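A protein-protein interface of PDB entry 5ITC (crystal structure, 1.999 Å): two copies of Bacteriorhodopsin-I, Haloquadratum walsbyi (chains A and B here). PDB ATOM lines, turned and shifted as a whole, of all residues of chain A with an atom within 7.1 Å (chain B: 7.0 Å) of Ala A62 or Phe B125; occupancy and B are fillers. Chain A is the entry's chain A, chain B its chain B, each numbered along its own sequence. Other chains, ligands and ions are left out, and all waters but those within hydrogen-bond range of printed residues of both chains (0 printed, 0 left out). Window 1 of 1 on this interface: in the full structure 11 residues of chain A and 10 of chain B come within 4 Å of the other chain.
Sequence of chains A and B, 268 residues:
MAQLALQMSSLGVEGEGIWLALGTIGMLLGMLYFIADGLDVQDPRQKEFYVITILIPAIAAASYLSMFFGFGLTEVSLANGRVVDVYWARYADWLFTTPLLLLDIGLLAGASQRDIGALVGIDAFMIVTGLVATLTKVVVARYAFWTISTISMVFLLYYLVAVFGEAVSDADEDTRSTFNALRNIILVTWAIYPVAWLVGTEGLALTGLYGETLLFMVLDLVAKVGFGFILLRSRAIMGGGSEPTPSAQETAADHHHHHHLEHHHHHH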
ATOM      1  N   THR A  24     -25.239   7.667 -19.549  1.00  0.00           N
ATOM      2  CA  THR A  24     -24.420   7.137 -18.452  1.00  0.00           C
ATOM      3  C   THR A  24     -22.925   7.380 -18.692  1.00  0.00           C
ATOM      4  O   THR A  24     -22.210   8.063 -17.898  1.00  0.00           O
ATOM      5  CB  THR A  24     -24.670   5.608 -18.250  1.00  0.00           C
ATOM      6  OG1 THR A  24     -26.063   5.372 -18.038  1.00  0.00           O
ATOM      7  CG2 THR A  24     -23.930   5.135 -17.013  1.00  0.00           C
ATOM      8  N   MET A  27     -21.856  11.103 -18.644  1.00  0.00           N
ATOM      9  CA  MET A  27     -21.712  11.619 -17.283  1.00  0.00           C
ATOM     10  C   MET A  27     -20.469  11.067 -16.624  1.00  0.00           C
ATOM     11  O   MET A  27     -19.657  11.803 -16.065  1.00  0.00           O
ATOM     12  CB  MET A  27     -22.964  11.311 -16.454  1.00  0.00           C
ATOM     13  CG  MET A  27     -24.202  12.008 -16.996  1.00  0.00           C
ATOM     14  SD  MET A  27     -24.173  13.805 -16.834  1.00  0.00           S
ATOM     15  CE  MET A  27     -25.784  14.162 -17.550  1.00  0.00           C
ATOM     16  N   MET A  31     -17.411  13.226 -15.237  1.00  0.00           N
ATOM     17  CA  MET A  31     -16.956  13.082 -13.849  1.00  0.00           C
ATOM     18  C   MET A  31     -15.466  12.743 -13.732  1.00  0.00           C
ATOM     19  O   MET A  31     -14.714  13.437 -12.995  1.00  0.00           O
ATOM     20  CB  MET A  31     -17.793  12.014 -13.127  1.00  0.00           C
ATOM     21  CG  MET A  31     -17.630  11.952 -11.605  1.00  0.00           C
ATOM     22  SD  MET A  31     -18.147  10.320 -10.956  1.00  0.00           S
ATOM     23  CE  MET A  31     -16.964   9.222 -11.714  1.00  0.00           C
ATOM     24  N   LEU A  55     -19.708  15.808  -7.931  1.00  0.00           N
ATOM     25  CA  LEU A  55     -20.923  15.184  -7.402  1.00  0.00           C
ATOM     26  C   LEU A  55     -22.084  15.241  -8.387  1.00  0.00           C
ATOM     27  O   LEU A  55     -22.800  14.252  -8.529  1.00  0.00           O
ATOM     28  CB  LEU A  55     -21.343  15.856  -6.087  1.00  0.00           C
ATOM     29  CG  LEU A  55     -22.417  15.112  -5.296  1.00  0.00           C
ATOM     30  CD1 LEU A  55     -22.068  13.615  -5.006  1.00  0.00           C
ATOM     31  CD2 LEU A  55     -22.730  15.888  -4.003  1.00  0.00           C
ATOM     32  N   ILE A  56     -22.232  16.360  -9.110  1.00  0.00           N
ATOM     33  CA  ILE A  56     -23.321  16.472 -10.090  1.00  0.00           C
ATOM     34  C   ILE A  56     -23.394  15.334 -11.195  1.00  0.00           C
ATOM     35  O   ILE A  56     -24.425  14.628 -11.365  1.00  0.00           O
ATOM     36  CB  ILE A  56     -23.309  17.887 -10.732  1.00  0.00           C
ATOM     37  CG1 ILE A  56     -23.881  18.896  -9.736  1.00  0.00           C
ATOM     38  CG2 ILE A  56     -24.243  17.947 -11.967  1.00  0.00           C
ATOM     39  CD1 ILE A  56     -23.420  20.357  -9.961  1.00  0.00           C
ATOM     40  N   PRO A  57     -22.317  15.167 -11.961  1.00  0.00           N
ATOM     41  CA  PRO A  57     -22.375  14.054 -12.919  1.00  0.00           C
ATOM     42  C   PRO A  57     -22.277  12.704 -12.244  1.00  0.00           C
ATOM     43  O   PRO A  57     -22.738  11.787 -12.882  1.00  0.00           O
ATOM     44  CB  PRO A  57     -21.144  14.262 -13.811  1.00  0.00           C
ATOM     45  CG  PRO A  57     -20.192  15.114 -12.956  1.00  0.00           C
ATOM     46  CD  PRO A  57     -21.068  15.946 -12.074  1.00  0.00           C
ATOM     47  N   ALA A  58     -21.651  12.534 -11.070  1.00  0.00           N
ATOM     48  CA  ALA A  58     -21.833  11.243 -10.370  1.00  0.00           C
ATOM     49  C   ALA A  58     -23.312  10.798 -10.159  1.00  0.00           C
ATOM     50  O   ALA A  58     -23.706   9.666 -10.467  1.00  0.00           O
ATOM     51  CB  ALA A  58     -21.135  11.278  -9.012  1.00  0.00           C
ATOM     52  N   ILE A  59     -24.101  11.701  -9.598  1.00  0.00           N
ATOM     53  CA  ILE A  59     -25.524  11.461  -9.333  1.00  0.00           C
ATOM     54  C   ILE A  59     -26.248  11.216 -10.664  1.00  0.00           C
ATOM     55  O   ILE A  59     -27.007  10.262 -10.791  1.00  0.00           O
ATOM     56  CB  ILE A  59     -26.145  12.662  -8.637  1.00  0.00           C
ATOM     57  CG1 ILE A  59     -25.460  12.938  -7.274  1.00  0.00           C
ATOM     58  CG2 ILE A  59     -27.693  12.610  -8.682  1.00  0.00           C
ATOM     59  CD1 ILE A  59     -25.729  14.351  -6.719  1.00  0.00           C
ATOM     60  N   ALA A  60     -25.928  12.025 -11.678  1.00  0.00           N
ATOM     61  CA  ALA A  60     -26.592  11.824 -12.958  1.00  0.00           C
ATOM     62  C   ALA A  60     -26.192  10.510 -13.639  1.00  0.00           C
ATOM     63  O   ALA A  60     -27.051   9.850 -14.214  1.00  0.00           O
ATOM     64  CB  ALA A  60     -26.227  13.011 -13.930  1.00  0.00           C
ATOM     65  N   ALA A  61     -24.926  10.096 -13.499  1.00  0.00           N
ATOM     66  CA  ALA A  61     -24.489   8.836 -14.081  1.00  0.00           C
ATOM     67  C   ALA A  61     -25.213   7.695 -13.391  1.00  0.00           C
ATOM     68  O   ALA A  61     -25.641   6.758 -14.027  1.00  0.00           O
ATOM     69  CB  ALA A  61     -23.020   8.646 -13.940  1.00  0.00           C
ATOM     70  N   ALA A  62     -25.289   7.764 -12.066  1.00  0.00           N
ATOM     71  CA  ALA A  62     -25.974   6.707 -11.337  1.00  0.00           C
ATOM     72  C   ALA A  62     -27.490   6.609 -11.668  1.00  0.00           C
ATOM     73  O   ALA A  62     -28.016   5.506 -11.884  1.00  0.00           O
ATOM     74  CB  ALA A  62     -25.727   6.888  -9.792  1.00  0.00           C
ATOM     75  N   SER A  63     -28.149   7.768 -11.805  1.00  0.00           N
ATOM     76  CA  SER A  63     -29.554   7.808 -12.230  1.00  0.00           C
ATOM     77  C   SER A  63     -29.707   7.207 -13.625  1.00  0.00           C
ATOM     78  O   SER A  63     -30.547   6.351 -13.822  1.00  0.00           O
ATOM     79  CB  SER A  63     -30.103   9.242 -12.216  1.00  0.00           C
ATOM     80  OG  SER A  63     -31.379   9.313 -12.851  1.00  0.00           O
ATOM     81  N   TYR A  64     -28.869   7.646 -14.559  1.00  0.00           N
ATOM     82  CA  TYR A  64     -28.881   7.125 -15.904  1.00  0.00           C
ATOM     83  C   TYR A  64     -28.678   5.616 -15.887  1.00  0.00           C
ATOM     84  O   TYR A  64     -29.349   4.918 -16.607  1.00  0.00           O
ATOM     85  CB  TYR A  64     -27.856   7.847 -16.812  1.00  0.00           C
ATOM     86  CG  TYR A  64     -28.509   9.002 -17.550  1.00  0.00           C
ATOM     87  CD1 TYR A  64     -28.731  10.222 -16.937  1.00  0.00           C
ATOM     88  CD2 TYR A  64     -29.010   8.822 -18.844  1.00  0.00           C
ATOM     89  CE1 TYR A  64     -29.404  11.253 -17.621  1.00  0.00           C
ATOM     90  CE2 TYR A  64     -29.658   9.847 -19.524  1.00  0.00           C
ATOM     91  CZ  TYR A  64     -29.848  11.059 -18.907  1.00  0.00           C
ATOM     92  OH  TYR A  64     -30.498  12.076 -19.584  1.00  0.00           O
ATOM     93  N   LEU A  65     -27.726   5.104 -15.128  1.00  0.00           N
ATOM     94  CA  LEU A  65     -27.513   3.640 -15.121  1.00  0.00           C
ATOM     95  C   LEU A  65     -28.775   2.918 -14.589  1.00  0.00           C
ATOM     96  O   LEU A  65     -29.185   1.852 -15.150  1.00  0.00           O
ATOM     97  CB  LEU A  65     -26.280   3.283 -14.289  1.00  0.00           C
ATOM     98  CG  LEU A  65     -25.820   1.830 -14.352  1.00  0.00           C
ATOM     99  CD1 LEU A  65     -25.494   1.420 -15.809  1.00  0.00           C
ATOM    100  CD2 LEU A  65     -24.638   1.579 -13.399  1.00  0.00           C
ATOM    101  N   SER A  66     -29.401   3.472 -13.536  1.00  0.00           N
ATOM    102  CA  SER A  66     -30.634   2.860 -12.957  1.00  0.00           C
ATOM    103  C   SER A  66     -31.708   2.845 -14.060  1.00  0.00           C
ATOM    104  O   SER A  66     -32.564   1.914 -14.138  1.00  0.00           O
ATOM    105  CB  SER A  66     -31.143   3.591 -11.698  1.00  0.00           C
ATOM    106  OG  SER A  66     -31.702   4.875 -11.997  1.00  0.00           O
ATOM    107  N   MET A  67     -31.767   3.916 -14.849  1.00  0.00           N
ATOM    108  CA  MET A  67     -32.821   3.966 -15.865  1.00  0.00           C
ATOM    109  C   MET A  67     -32.505   2.999 -16.993  1.00  0.00           C
ATOM    110  O   MET A  67     -33.401   2.348 -17.532  1.00  0.00           O
ATOM    111  CB  MET A  67     -32.955   5.369 -16.449  1.00  0.00           C
ATOM    112  CG  MET A  67     -33.361   6.388 -15.442  1.00  0.00           C
ATOM    113  SD  MET A  67     -33.732   7.971 -16.191  1.00  0.00           S
ATOM    114  CE  MET A  67     -32.130   8.764 -16.039  1.00  0.00           C
ATOM    115  N   PHE A  68     -31.211   2.866 -17.310  1.00  0.00           N
ATOM    116  CA  PHE A  68     -30.796   1.914 -18.331  1.00  0.00           C
ATOM    117  C   PHE A  68     -31.166   0.497 -17.942  1.00  0.00           C
ATOM    118  O   PHE A  68     -31.574  -0.304 -18.793  1.00  0.00           O
ATOM    119  CB  PHE A  68     -29.278   1.977 -18.576  1.00  0.00           C
ATOM    120  CG  PHE A  68     -28.767   0.826 -19.441  1.00  0.00           C
ATOM    121  CD1 PHE A  68     -28.931   0.869 -20.831  1.00  0.00           C
ATOM    122  CD2 PHE A  68     -28.242  -0.321 -18.866  1.00  0.00           C
ATOM    123  CE1 PHE A  68     -28.486  -0.166 -21.645  1.00  0.00           C
ATOM    124  CE2 PHE A  68     -27.826  -1.378 -19.656  1.00  0.00           C
ATOM    125  CZ  PHE A  68     -27.943  -1.312 -21.048  1.00  0.00           C
ATOM    126  N   PHE A  69     -31.092   0.192 -16.647  1.00  0.00           N
ATOM    127  CA  PHE A  69     -31.395  -1.177 -16.251  1.00  0.00           C
ATOM    128  C   PHE A  69     -32.901  -1.355 -16.019  1.00  0.00           C
ATOM    129  O   PHE A  69     -33.366  -2.482 -15.977  1.00  0.00           O
ATOM    130  CB  PHE A  69     -30.680  -1.554 -14.929  1.00  0.00           C
ATOM    131  CG  PHE A  69     -29.233  -1.822 -15.048  1.00  0.00           C
ATOM    132  CD1 PHE A  69     -28.777  -2.845 -15.854  1.00  0.00           C
ATOM    133  CD2 PHE A  69     -28.333  -1.160 -14.239  1.00  0.00           C
ATOM    134  CE1 PHE A  69     -27.430  -3.129 -15.932  1.00  0.00           C
ATOM    135  CE2 PHE A  69     -26.988  -1.436 -14.308  1.00  0.00           C
ATOM    136  CZ  PHE A  69     -26.530  -2.420 -15.157  1.00  0.00           C
ATOM    137  N   ALA A  89     -36.796   8.309 -12.267  1.00  0.00           N
ATOM    138  CA  ALA A  89     -35.463   8.538 -11.676  1.00  0.00           C
ATOM    139  C   ALA A  89     -34.818   9.876 -12.016  1.00  0.00           C
ATOM    140  O   ALA A  89     -34.047  10.428 -11.199  1.00  0.00           O
ATOM    141  CB  ALA A  89     -34.530   7.394 -12.070  1.00  0.00           C
ATOM    142  N   ASP A  93     -32.820  12.421  -9.645  1.00  0.00           N
ATOM    143  CA  ASP A  93     -31.588  13.090 -10.040  1.00  0.00           C
ATOM    144  C   ASP A  93     -31.738  14.633  -9.898  1.00  0.00           C
ATOM    145  O   ASP A  93     -30.991  15.277  -9.117  1.00  0.00           O
ATOM    146  CB  ASP A  93     -31.201  12.585 -11.433  1.00  0.00           C
ATOM    147  CG  ASP A  93     -30.141  13.443 -12.172  1.00  0.00           C
ATOM    148  OD1 ASP A  93     -29.563  14.416 -11.654  1.00  0.00           O
ATOM    149  OD2 ASP A  93     -29.842  13.044 -13.309  1.00  0.00           O
ATOM    150  N   LEU B  95     -30.047   6.883   5.832  1.00  0.00           N
ATOM    151  CA  LEU B  95     -29.949   8.120   5.050  1.00  0.00           C
ATOM    152  C   LEU B  95     -29.735   9.360   5.914  1.00  0.00           C
ATOM    153  O   LEU B  95     -29.122  10.356   5.472  1.00  0.00           O
ATOM    154  CB  LEU B  95     -31.187   8.293   4.179  1.00  0.00           C
ATOM    155  CG  LEU B  95     -31.028   9.372   3.111  1.00  0.00           C
ATOM    156  CD1 LEU B  95     -29.786   9.131   2.252  1.00  0.00           C
ATOM    157  CD2 LEU B  95     -32.280   9.369   2.246  1.00  0.00           C
ATOM    158  N   LEU B 119     -18.185  15.307   2.678  1.00  0.00           N
ATOM    159  CA  LEU B 119     -18.379  13.902   3.104  1.00  0.00           C
ATOM    160  C   LEU B 119     -19.828  13.503   3.206  1.00  0.00           C
ATOM    161  O   LEU B 119     -20.140  12.365   2.941  1.00  0.00           O
ATOM    162  CB  LEU B 119     -17.756  13.519   4.439  1.00  0.00           C
ATOM    163  CG  LEU B 119     -16.318  13.135   4.644  1.00  0.00           C
ATOM    164  CD1 LEU B 119     -16.145  12.530   6.022  1.00  0.00           C
ATOM    165  CD2 LEU B 119     -16.064  12.022   3.587  1.00  0.00           C
ATOM    166  N   VAL B 120     -20.684  14.407   3.646  1.00  0.00           N
ATOM    167  CA  VAL B 120     -22.109  14.129   3.728  1.00  0.00           C
ATOM    168  C   VAL B 120     -22.613  13.847   2.273  1.00  0.00           C
ATOM    169  O   VAL B 120     -23.472  12.998   2.065  1.00  0.00           O
ATOM    170  CB  VAL B 120     -22.875  15.304   4.407  1.00  0.00           C
ATOM    171  CG1 VAL B 120     -24.350  15.188   4.175  1.00  0.00           C
ATOM    172  CG2 VAL B 120     -22.589  15.329   5.937  1.00  0.00           C
ATOM    173  N   GLY B 121     -22.192  14.666   1.309  1.00  0.00           N
ATOM    174  CA  GLY B 121     -22.460  14.439  -0.113  1.00  0.00           C
ATOM    175  C   GLY B 121     -22.157  12.996  -0.516  1.00  0.00           C
ATOM    176  O   GLY B 121     -22.979  12.268  -1.163  1.00  0.00           O
ATOM    177  N   ILE B 122     -20.937  12.581  -0.164  1.00  0.00           N
ATOM    178  CA  ILE B 122     -20.520  11.250  -0.629  1.00  0.00           C
ATOM    179  C   ILE B 122     -21.185  10.109   0.115  1.00  0.00           C
ATOM    180  O   ILE B 122     -21.559   9.092  -0.476  1.00  0.00           O
ATOM    181  CB  ILE B 122     -18.991  11.077  -0.337  1.00  0.00           C
ATOM    182  CG1 ILE B 122     -18.176  12.019  -1.203  1.00  0.00           C
ATOM    183  CG2 ILE B 122     -18.533   9.622  -0.460  1.00  0.00           C
ATOM    184  CD1 ILE B 122     -16.841  12.246  -0.620  1.00  0.00           C
ATOM    185  N   ASP B 123     -21.462  10.348   1.395  1.00  0.00           N
ATOM    186  CA  ASP B 123     -22.274   9.461   2.201  1.00  0.00           C
ATOM    187  C   ASP B 123     -23.697   9.241   1.661  1.00  0.00           C
ATOM    188  O   ASP B 123     -24.203   8.108   1.650  1.00  0.00           O
ATOM    189  CB  ASP B 123     -22.325   9.978   3.628  1.00  0.00           C
ATOM    190  CG  ASP B 123     -23.079   9.009   4.531  1.00  0.00           C
ATOM    191  OD1 ASP B 123     -24.332   9.126   4.558  1.00  0.00           O
ATOM    192  OD2 ASP B 123     -22.452   8.116   5.131  1.00  0.00           O
ATOM    193  N   ALA B 124     -24.358  10.338   1.284  1.00  0.00           N
ATOM    194  CA  ALA B 124     -25.721  10.248   0.787  1.00  0.00           C
ATOM    195  C   ALA B 124     -25.676   9.407  -0.502  1.00  0.00           C
ATOM    196  O   ALA B 124     -26.536   8.530  -0.737  1.00  0.00           O
ATOM    197  CB  ALA B 124     -26.306  11.645   0.516  1.00  0.00           C
ATOM    198  N   PHE B 125     -24.703   9.748  -1.374  1.00  0.00           N
ATOM    199  CA  PHE B 125     -24.519   8.987  -2.617  1.00  0.00           C
ATOM    200  C   PHE B 125     -24.386   7.450  -2.319  1.00  0.00           C
ATOM    201  O   PHE B 125     -25.064   6.590  -2.936  1.00  0.00           O
ATOM    202  CB  PHE B 125     -23.300   9.491  -3.382  1.00  0.00           C
ATOM    203  CG  PHE B 125     -23.118   8.833  -4.725  1.00  0.00           C
ATOM    204  CD1 PHE B 125     -23.797   9.313  -5.835  1.00  0.00           C
ATOM    205  CD2 PHE B 125     -22.314   7.724  -4.870  1.00  0.00           C
ATOM    206  CE1 PHE B 125     -23.648   8.704  -7.105  1.00  0.00           C
ATOM    207  CE2 PHE B 125     -22.154   7.103  -6.134  1.00  0.00           C
ATOM    208  CZ  PHE B 125     -22.835   7.599  -7.239  1.00  0.00           C
ATOM    209  N   MET B 126     -23.539   7.113  -1.333  1.00  0.00           N
ATOM    210  CA  MET B 126     -23.352   5.708  -0.900  1.00  0.00           C
ATOM    211  C   MET B 126     -24.653   5.031  -0.421  1.00  0.00           C
ATOM    212  O   MET B 126     -24.982   3.908  -0.868  1.00  0.00           O
ATOM    213  CB  MET B 126     -22.350   5.652   0.251  1.00  0.00           C
ATOM    214  CG  MET B 126     -22.141   4.269   0.873  1.00  0.00           C
ATOM    215  SD  MET B 126     -21.036   4.379   2.332  1.00  0.00           S
ATOM    216  CE  MET B 126     -22.187   4.960   3.580  1.00  0.00           C
ATOM    217  N   ILE B 127     -25.422   5.713   0.440  1.00  0.00           N
ATOM    218  CA  ILE B 127     -26.690   5.115   0.936  1.00  0.00           C
ATOM    219  C   ILE B 127     -27.742   4.926  -0.178  1.00  0.00           C
ATOM    220  O   ILE B 127     -28.394   3.858  -0.259  1.00  0.00           O
ATOM    221  CB  ILE B 127     -27.318   5.948   2.068  1.00  0.00           C
ATOM    222  CG1 ILE B 127     -26.328   6.039   3.249  1.00  0.00           C
ATOM    223  CG2 ILE B 127     -28.709   5.349   2.537  1.00  0.00           C
ATOM    224  CD1 ILE B 127     -25.794   4.646   3.755  1.00  0.00           C
ATOM    225  N   VAL B 128     -27.976   5.978  -0.957  1.00  0.00           N
ATOM    226  CA  VAL B 128     -28.927   5.930  -2.072  1.00  0.00           C
ATOM    227  C   VAL B 128     -28.551   4.830  -3.114  1.00  0.00           C
ATOM    228  O   VAL B 128     -29.418   4.055  -3.563  1.00  0.00           O
ATOM    229  CB  VAL B 128     -28.995   7.291  -2.756  1.00  0.00           C
ATOM    230  CG1 VAL B 128     -29.936   7.230  -3.963  1.00  0.00           C
ATOM    231  CG2 VAL B 128     -29.573   8.344  -1.758  1.00  0.00           C
ATOM    232  N   THR B 129     -27.273   4.735  -3.483  1.00  0.00           N
ATOM    233  CA  THR B 129     -26.873   3.727  -4.477  1.00  0.00           C
ATOM    234  C   THR B 129     -27.023   2.343  -3.830  1.00  0.00           C
ATOM    235  O   THR B 129     -27.398   1.383  -4.514  1.00  0.00           O
ATOM    236  CB  THR B 129     -25.421   3.963  -5.056  1.00  0.00           C
ATOM    237  OG1 THR B 129     -24.495   4.228  -3.981  1.00  0.00           O
ATOM    238  CG2 THR B 129     -25.430   5.194  -5.987  1.00  0.00           C
ATOM    239  N   GLY B 130     -26.781   2.231  -2.521  1.00  0.00           N
ATOM    240  CA  GLY B 130     -27.054   0.959  -1.866  1.00  0.00           C
ATOM    241  C   GLY B 130     -28.545   0.547  -1.854  1.00  0.00           C
ATOM    242  O   GLY B 130     -28.910  -0.616  -2.055  1.00  0.00           O
ATOM    243  N   LEU B 131     -29.430   1.524  -1.670  1.00  0.00           N
ATOM    244  CA  LEU B 131     -30.879   1.284  -1.787  1.00  0.00           C
ATOM    245  C   LEU B 131     -31.281   0.847  -3.208  1.00  0.00           C
ATOM    246  O   LEU B 131     -32.085  -0.092  -3.399  1.00  0.00           O
ATOM    247  CB  LEU B 131     -31.649   2.556  -1.404  1.00  0.00           C
ATOM    248  CG  LEU B 131     -33.174   2.401  -1.516  1.00  0.00           C
ATOM    249  CD1 LEU B 131     -33.717   1.344  -0.552  1.00  0.00           C
ATOM    250  CD2 LEU B 131     -33.834   3.741  -1.294  1.00  0.00           C
ATOM    251  N   VAL B 132     -30.682   1.496  -4.208  1.00  0.00           N
ATOM    252  CA  VAL B 132     -30.951   1.066  -5.575  1.00  0.00           C
ATOM    253  C   VAL B 132     -30.487  -0.415  -5.720  1.00  0.00           C
ATOM    254  O   VAL B 132     -31.230  -1.240  -6.208  1.00  0.00           O
ATOM    255  CB  VAL B 132     -30.260   1.954  -6.623  1.00  0.00           C
ATOM    256  CG1 VAL B 132     -30.557   1.383  -8.077  1.00  0.00           C
ATOM    257  CG2 VAL B 132     -30.788   3.400  -6.517  1.00  0.00           C
ATOM    258  N   PHE B 145     -24.658  -1.784  -8.679  1.00  0.00           N
ATOM    259  CA  PHE B 145     -24.922  -0.715  -7.700  1.00  0.00           C
ATOM    260  C   PHE B 145     -24.225  -0.976  -6.392  1.00  0.00           C
ATOM    261  O   PHE B 145     -23.819  -0.025  -5.736  1.00  0.00           O
ATOM    262  CB  PHE B 145     -26.420  -0.427  -7.550  1.00  0.00           C
ATOM    263  CG  PHE B 145     -26.885   0.504  -8.608  1.00  0.00           C
ATOM    264  CD1 PHE B 145     -26.801   1.873  -8.375  1.00  0.00           C
ATOM    265  CD2 PHE B 145     -27.304   0.040  -9.867  1.00  0.00           C
ATOM    266  CE1 PHE B 145     -27.177   2.781  -9.375  1.00  0.00           C
ATOM    267  CE2 PHE B 145     -27.664   0.917 -10.856  1.00  0.00           C
ATOM    268  CZ  PHE B 145     -27.583   2.300 -10.621  1.00  0.00           C
ATOM    269  N   ILE B 148     -20.752   0.268  -7.063  1.00  0.00           N
ATOM    270  CA  ILE B 148     -20.736   1.723  -7.019  1.00  0.00           C
ATOM    271  C   ILE B 148     -20.758   2.244  -5.548  1.00  0.00           C
ATOM    272  O   ILE B 148     -19.972   3.157  -5.120  1.00  0.00           O
ATOM    273  CB  ILE B 148     -21.918   2.260  -7.851  1.00  0.00           C
ATOM    274  CG1 ILE B 148     -21.614   1.978  -9.328  1.00  0.00           C
ATOM    275  CG2 ILE B 148     -22.138   3.777  -7.590  1.00  0.00           C
ATOM    276  CD1 ILE B 148     -22.803   2.072 -10.314  1.00  0.00           C
ATOM    277  N   SER B 149     -21.656   1.645  -4.767  1.00  0.00           N
ATOM    278  CA  SER B 149     -21.832   2.084  -3.362  1.00  0.00           C
ATOM    279  C   SER B 149     -20.577   1.798  -2.536  1.00  0.00           C
ATOM    280  O   SER B 149     -20.113   2.640  -1.762  1.00  0.00           O
ATOM    281  CB  SER B 149     -23.075   1.397  -2.749  1.00  0.00           C
ATOM    282  OG  SER B 149     -23.286   1.808  -1.392  1.00  0.00           O
ATOM    283  N   SER B 152     -17.824   4.280  -3.362  1.00  0.00           N
ATOM    284  CA  SER B 152     -18.103   5.492  -2.591  1.00  0.00           C
ATOM    285  C   SER B 152     -17.720   5.347  -1.138  1.00  0.00           C
ATOM    286  O   SER B 152     -17.185   6.285  -0.566  1.00  0.00           O
ATOM    287  CB  SER B 152     -19.589   5.864  -2.687  1.00  0.00           C
ATOM    288  OG  SER B 152     -20.034   5.648  -3.990  1.00  0.00           O
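Phe B125 touches just these residues of chain A: Ala A58, Ile A59 and Ala A62.
Of the printed residues of chain B, Ala A58 touches Phe B125 (3.5 Å).
Printed residues of chain A within 4 Å of Phe B145: Ala A62 and Ser A66.
Val B132 touches none of the printed residues of chain A.
Ser B149 touches none of the printed residues of chain A.
The nearest residue of chain A that does not touch Phe B125 is Leu A55 (4.6 Å).
The nearest printed residue of chain B that does not touch Leu A65 is Phe B145 (4.01 Å).
The backbone carbonyl oxygen (O) of Ser A63 lies within hydrogen-bond range of the side-chain hydroxyl (OG) of Ser A66 (2.6 Å).
The backbone carbonyl oxygen (O) of Ile B148 sits at hydrogen-bond distance from the side-chain hydroxyl (OG) of Ser B152 (2.7 Å).
OG1 of Thr B129 is in hydrogen-bond range of O of Phe B125, 2.6 Å away.
The side-chain hydroxyl (OG1) of Thr A24 is in hydrogen-bond range of the backbone NH (N) of Leu A65, at 3.4 Å.
No position is printed for both chains.
Of the 6 pairs that touch across the chains among the printed residues, none has its exchanged pair printed and touching as well.
Of the 20 printed residues of chain A, 5 touch a printed residue of chain B.
Printed residues of chain A that touch a printed residue of chain B: Ala A58, Ile A59, Ala A62, Leu A65 and Ser A66.
Hydrophobic or aromatic side chains of chain A that line the printed part of chain B: Ala A62 and Leu A65.
Along chain B the printed residues that touch a printed residue of chain A span positions 125 to 148.
Among the printed residues, 6 pairs touch across the chains.
Among the printed residues, no Asp or Glu carboxylate lies within 4 Å of a Lys or Arg side-chain nitrogen of the other chain.
Among the printed residues, pairs that only touch across the chains: Ala A62 with Phe B145 (3.5 Å), Ala A58 with Phe B125 (3.5 Å), Leu A65 with Ile B148 (3.6 Å), Ser A66 with Phe B145 (3.6 Å), Ala A62 with Phe B125 (3.9 Å) and Ile A59 with Phe B125 (3.9 Å).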
